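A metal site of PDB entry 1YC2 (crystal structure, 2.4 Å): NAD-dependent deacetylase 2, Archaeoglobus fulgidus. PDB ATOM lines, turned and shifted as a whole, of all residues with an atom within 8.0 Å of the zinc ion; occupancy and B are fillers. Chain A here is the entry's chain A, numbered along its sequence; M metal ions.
Four residues have an atom within 4 Å of the zinc ion: Cys 126, Cys 129, Cys 150 and Cys 153.
The zinc ion is bound by the side-chain sulfur (SG) of Cys 129 (2.4 Å), the side-chain sulfur (SG) of Cys 150 (2.4 Å), the side-chain sulfur (SG) of Cys 153 (2.4 Å) and the side-chain sulfur (SG) of Cys 126 (2.4 Å).
The zinc ion has four donor atoms within binding distance.
The side-chain sulfur of Cys 129 lies close to the backbone NH of Glu 131, at 3.5 Å.
The backbone NH of Cys 150 is in hydrogen-bond range of the backbone carbonyl oxygen of Ser 155 (2.8 Å).
SG of Cys 150 lies close to N of Lys 152 (3.5 Å).
SG of Cys 150 sits close to OH of Tyr 133 (3.2 Å).
SG of Cys 153 lies close to N of Ser 155 (3.3 Å).
N of Cys 126 sits at hydrogen-bond distance from O of Glu 131, at 2.9 Å.
The side-chain sulfur of Cys 126 sits close to the backbone NH of Asp 128, at 3.4 Å.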
ATOM      1  N   ASP A 125      -4.919  21.977   7.826  1.00  0.00           N
ATOM      2  CA  ASP A 125      -4.203  21.359   6.720  1.00  0.00           C
ATOM      3  C   ASP A 125      -2.792  21.937   6.577  1.00  0.00           C
ATOM      4  O   ASP A 125      -2.596  23.146   6.674  1.00  0.00           O
ATOM      5  CB  ASP A 125      -4.926  21.585   5.388  1.00  0.00           C
ATOM      6  CG  ASP A 125      -6.329  21.034   5.370  1.00  0.00           C
ATOM      7  OD1 ASP A 125      -6.490  19.798   5.409  1.00  0.00           O
ATOM      8  OD2 ASP A 125      -7.284  21.846   5.328  1.00  0.00           O
ATOM      9  N   CYS A 126      -1.820  21.072   6.347  1.00  0.00           N
ATOM     10  CA  CYS A 126      -0.471  21.541   6.125  1.00  0.00           C
ATOM     11  C   CYS A 126      -0.477  21.951   4.650  1.00  0.00           C
ATOM     12  O   CYS A 126      -0.879  21.148   3.805  1.00  0.00           O
ATOM     13  CB  CYS A 126       0.548  20.411   6.334  1.00  0.00           C
ATOM     14  SG  CYS A 126       2.211  20.882   5.788  1.00  0.00           S
ATOM     15  N   LEU A 127      -0.042  23.172   4.350  1.00  0.00           N
ATOM     16  CA  LEU A 127      -0.042  23.636   2.959  1.00  0.00           C
ATOM     17  C   LEU A 127       1.083  23.046   2.120  1.00  0.00           C
ATOM     18  O   LEU A 127       1.041  23.136   0.903  1.00  0.00           O
ATOM     19  CB  LEU A 127       0.050  25.173   2.885  1.00  0.00           C
ATOM     20  CG  LEU A 127      -1.153  26.026   3.277  1.00  0.00           C
ATOM     21  CD1 LEU A 127      -2.441  25.379   2.784  1.00  0.00           C
ATOM     22  CD2 LEU A 127      -1.209  26.168   4.773  1.00  0.00           C
ATOM     23  N   ASP A 128       2.088  22.454   2.760  1.00  0.00           N
ATOM     24  CA  ASP A 128       3.212  21.883   2.014  1.00  0.00           C
ATOM     25  C   ASP A 128       3.045  20.414   1.639  1.00  0.00           C
ATOM     26  O   ASP A 128       3.220  20.056   0.472  1.00  0.00           O
ATOM     27  CB  ASP A 128       4.531  22.064   2.768  1.00  0.00           C
ATOM     28  CG  ASP A 128       4.963  23.519   2.858  1.00  0.00           C
ATOM     29  OD1 ASP A 128       4.906  24.237   1.835  1.00  0.00           O
ATOM     30  OD2 ASP A 128       5.391  23.952   3.943  1.00  0.00           O
ATOM     31  N   CYS A 129       2.705  19.572   2.609  1.00  0.00           N
ATOM     32  CA  CYS A 129       2.563  18.148   2.329  1.00  0.00           C
ATOM     33  C   CYS A 129       1.113  17.639   2.254  1.00  0.00           C
ATOM     34  O   CYS A 129       0.877  16.507   1.835  1.00  0.00           O
ATOM     35  CB  CYS A 129       3.348  17.325   3.357  1.00  0.00           C
ATOM     36  SG  CYS A 129       2.448  16.971   4.857  1.00  0.00           S
ATOM     37  N   HIS A 130       0.169  18.468   2.680  1.00  0.00           N
ATOM     38  CA  HIS A 130      -1.253  18.127   2.635  1.00  0.00           C
ATOM     39  C   HIS A 130      -1.765  17.211   3.724  1.00  0.00           C
ATOM     40  O   HIS A 130      -2.816  16.585   3.586  1.00  0.00           O
ATOM     41  CB  HIS A 130      -1.624  17.546   1.273  1.00  0.00           C
ATOM     42  CG  HIS A 130      -1.210  18.431   0.147  1.00  0.00           C
ATOM     43  ND1 HIS A 130      -1.627  19.737   0.051  1.00  0.00           N
ATOM     44  CD2 HIS A 130      -0.347  18.230  -0.877  1.00  0.00           C
ATOM     45  CE1 HIS A 130      -1.038  20.309  -0.984  1.00  0.00           C
ATOM     46  NE2 HIS A 130      -0.254  19.417  -1.553  1.00  0.00           N
ATOM     47  N   GLU A 131      -1.023  17.116   4.815  1.00  0.00           N
ATOM     48  CA  GLU A 131      -1.461  16.296   5.928  1.00  0.00           C
ATOM     49  C   GLU A 131      -2.622  17.059   6.563  1.00  0.00           C
ATOM     50  O   GLU A 131      -2.629  18.294   6.562  1.00  0.00           O
ATOM     51  CB  GLU A 131      -0.340  16.124   6.945  1.00  0.00           C
ATOM     52  CG  GLU A 131      -0.596  15.061   7.992  1.00  0.00           C
ATOM     53  CD  GLU A 131      -0.741  13.689   7.376  1.00  0.00           C
ATOM     54  OE1 GLU A 131      -0.068  13.430   6.356  1.00  0.00           O
ATOM     55  OE2 GLU A 131      -1.520  12.865   7.919  1.00  0.00           O
ATOM     56  N   THR A 132      -3.610  16.344   7.079  1.00  0.00           N
ATOM     57  CA  THR A 132      -4.713  17.017   7.747  1.00  0.00           C
ATOM     58  C   THR A 132      -4.691  16.578   9.203  1.00  0.00           C
ATOM     59  O   THR A 132      -4.262  15.473   9.510  1.00  0.00           O
ATOM     60  CB  THR A 132      -6.082  16.674   7.132  1.00  0.00           C
ATOM     61  OG1 THR A 132      -6.395  15.314   7.413  1.00  0.00           O
ATOM     62  CG2 THR A 132      -6.045  16.876   5.634  1.00  0.00           C
ATOM     63  N   TYR A 133      -5.108  17.464  10.096  1.00  0.00           N
ATOM     64  CA  TYR A 133      -5.142  17.169  11.519  1.00  0.00           C
ATOM     65  C   TYR A 133      -6.434  17.676  12.099  1.00  0.00           C
ATOM     66  O   TYR A 133      -7.126  18.503  11.494  1.00  0.00           O
ATOM     67  CB  TYR A 133      -3.994  17.864  12.253  1.00  0.00           C
ATOM     68  CG  TYR A 133      -2.601  17.506  11.772  1.00  0.00           C
ATOM     69  CD1 TYR A 133      -1.948  18.272  10.793  1.00  0.00           C
ATOM     70  CD2 TYR A 133      -1.930  16.400  12.288  1.00  0.00           C
ATOM     71  CE1 TYR A 133      -0.667  17.932  10.355  1.00  0.00           C
ATOM     72  CE2 TYR A 133      -0.660  16.059  11.859  1.00  0.00           C
ATOM     73  CZ  TYR A 133      -0.029  16.824  10.897  1.00  0.00           C
ATOM     74  OH  TYR A 133       1.225  16.464  10.469  1.00  0.00           O
ATOM     75  N   ARG A 149       2.707  22.877  14.145  1.00  0.00           N
ATOM     76  CA  ARG A 149       3.693  22.542  13.116  1.00  0.00           C
ATOM     77  C   ARG A 149       3.440  21.138  12.589  1.00  0.00           C
ATOM     78  O   ARG A 149       3.132  20.237  13.352  1.00  0.00           O
ATOM     79  CB  ARG A 149       5.083  22.635  13.744  1.00  0.00           C
ATOM     80  CG  ARG A 149       6.221  22.285  12.841  1.00  0.00           C
ATOM     81  CD  ARG A 149       7.510  22.228  13.636  1.00  0.00           C
ATOM     82  NE  ARG A 149       8.667  22.011  12.771  1.00  0.00           N
ATOM     83  CZ  ARG A 149       9.897  21.772  13.216  1.00  0.00           C
ATOM     84  NH1 ARG A 149      10.886  21.590  12.358  1.00  0.00           N
ATOM     85  NH2 ARG A 149      10.129  21.727  14.521  1.00  0.00           N
ATOM     86  N   CYS A 150       3.574  20.951  11.283  1.00  0.00           N
ATOM     87  CA  CYS A 150       3.326  19.638  10.714  1.00  0.00           C
ATOM     88  C   CYS A 150       4.301  18.610  11.284  1.00  0.00           C
ATOM     89  O   CYS A 150       5.512  18.840  11.310  1.00  0.00           O
ATOM     90  CB  CYS A 150       3.452  19.689   9.190  1.00  0.00           C
ATOM     91  SG  CYS A 150       2.905  18.172   8.353  1.00  0.00           S
ATOM     92  N   ARG A 151       3.763  17.480  11.749  1.00  0.00           N
ATOM     93  CA  ARG A 151       4.564  16.412  12.320  1.00  0.00           C
ATOM     94  C   ARG A 151       5.132  15.496  11.248  1.00  0.00           C
ATOM     95  O   ARG A 151       6.002  14.673  11.540  1.00  0.00           O
ATOM     96  CB  ARG A 151       3.721  15.588  13.302  1.00  0.00           C
ATOM     97  CG  ARG A 151       3.450  16.281  14.645  1.00  0.00           C
ATOM     98  CD  ARG A 151       1.972  16.219  15.019  1.00  0.00           C
ATOM     99  NE  ARG A 151       1.667  16.802  16.328  1.00  0.00           N
ATOM    100  CZ  ARG A 151       2.065  18.009  16.745  1.00  0.00           C
ATOM    101  NH1 ARG A 151       2.800  18.790  15.966  1.00  0.00           N
ATOM    102  NH2 ARG A 151       1.691  18.443  17.938  1.00  0.00           N
ATOM    103  N   LYS A 152       4.651  15.645  10.014  1.00  0.00           N
ATOM    104  CA  LYS A 152       5.131  14.826   8.908  1.00  0.00           C
ATOM    105  C   LYS A 152       6.269  15.439   8.113  1.00  0.00           C
ATOM    106  O   LYS A 152       7.250  14.760   7.820  1.00  0.00           O
ATOM    107  CB  LYS A 152       3.976  14.499   7.958  1.00  0.00           C
ATOM    108  CG  LYS A 152       3.060  13.400   8.470  1.00  0.00           C
ATOM    109  CD  LYS A 152       3.846  12.121   8.687  1.00  0.00           C
ATOM    110  CE  LYS A 152       2.986  11.034   9.308  1.00  0.00           C
ATOM    111  NZ  LYS A 152       3.790   9.809   9.601  1.00  0.00           N
ATOM    112  N   CYS A 153       6.145  16.722   7.767  1.00  0.00           N
ATOM    113  CA  CYS A 153       7.181  17.391   6.997  1.00  0.00           C
ATOM    114  C   CYS A 153       7.822  18.523   7.791  1.00  0.00           C
ATOM    115  O   CYS A 153       8.777  19.164   7.341  1.00  0.00           O
ATOM    116  CB  CYS A 153       6.585  17.932   5.688  1.00  0.00           C
ATOM    117  SG  CYS A 153       5.693  19.486   5.869  1.00  0.00           S
ATOM    118  N   GLY A 154       7.283  18.789   8.974  1.00  0.00           N
ATOM    119  CA  GLY A 154       7.831  19.847   9.813  1.00  0.00           C
ATOM    120  C   GLY A 154       7.529  21.261   9.366  1.00  0.00           C
ATOM    121  O   GLY A 154       8.157  22.205   9.857  1.00  0.00           O
ATOM    122  N   SER A 155       6.599  21.436   8.433  1.00  0.00           N
ATOM    123  CA  SER A 155       6.239  22.774   7.962  1.00  0.00           C
ATOM    124  C   SER A 155       5.481  23.583   9.020  1.00  0.00           C
ATOM    125  O   SER A 155       4.843  23.015   9.899  1.00  0.00           O
ATOM    126  CB  SER A 155       5.380  22.676   6.700  1.00  0.00           C
ATOM    127  OG  SER A 155       4.861  23.939   6.316  1.00  0.00           O
ATOM    128  N   TYR A 156       5.573  24.905   8.936  1.00  0.00           N
ATOM    129  CA  TYR A 156       4.857  25.764   9.868  1.00  0.00           C
ATOM    130  C   TYR A 156       3.583  26.314   9.235  1.00  0.00           C
ATOM    131  O   TYR A 156       2.869  27.122   9.840  1.00  0.00           O
ATOM    132  CB  TYR A 156       5.728  26.930  10.325  1.00  0.00           C
ATOM    133  CG  TYR A 156       6.789  26.549  11.325  1.00  0.00           C
ATOM    134  CD1 TYR A 156       7.915  25.845  10.929  1.00  0.00           C
ATOM    135  CD2 TYR A 156       6.660  26.896  12.666  1.00  0.00           C
ATOM    136  CE1 TYR A 156       8.895  25.484  11.837  1.00  0.00           C
ATOM    137  CE2 TYR A 156       7.639  26.538  13.597  1.00  0.00           C
ATOM    138  CZ  TYR A 156       8.757  25.833  13.177  1.00  0.00           C
ATOM    139  OH  TYR A 156       9.745  25.506  14.078  1.00  0.00           O
ATOM    140  N   TYR A 157       3.284  25.897   8.005  1.00  0.00           N
ATOM    141  CA  TYR A 157       2.088  26.376   7.339  1.00  0.00           C
ATOM    142  C   TYR A 157       0.920  25.412   7.526  1.00  0.00           C
ATOM    143  O   TYR A 157       0.486  24.747   6.595  1.00  0.00           O
ATOM    144  CB  TYR A 157       2.366  26.592   5.842  1.00  0.00           C
ATOM    145  CG  TYR A 157       3.461  27.606   5.565  1.00  0.00           C
ATOM    146  CD1 TYR A 157       4.802  27.299   5.811  1.00  0.00           C
ATOM    147  CD2 TYR A 157       3.158  28.876   5.068  1.00  0.00           C
ATOM    148  CE1 TYR A 157       5.814  28.241   5.570  1.00  0.00           C
ATOM    149  CE2 TYR A 157       4.172  29.822   4.818  1.00  0.00           C
ATOM    150  CZ  TYR A 157       5.487  29.494   5.075  1.00  0.00           C
ATOM    151  OH  TYR A 157       6.484  30.426   4.871  1.00  0.00           O
ATOM    152  N   VAL A 158       0.445  25.326   8.768  1.00  0.00           N
ATOM    153  CA  VAL A 158      -0.679  24.457   9.081  1.00  0.00           C
ATOM    154  C   VAL A 158      -1.851  25.406   9.233  1.00  0.00           C
ATOM    155  O   VAL A 158      -2.017  26.053  10.266  1.00  0.00           O
ATOM    156  CB  VAL A 158      -0.442  23.668  10.386  1.00  0.00           C
ATOM    157  CG1 VAL A 158      -1.570  22.670  10.610  1.00  0.00           C
ATOM    158  CG2 VAL A 158       0.901  22.936  10.314  1.00  0.00           C
HETATM  159 ZN    ZN M   1       3.386  18.770   6.079  1.00  0.00          ZN
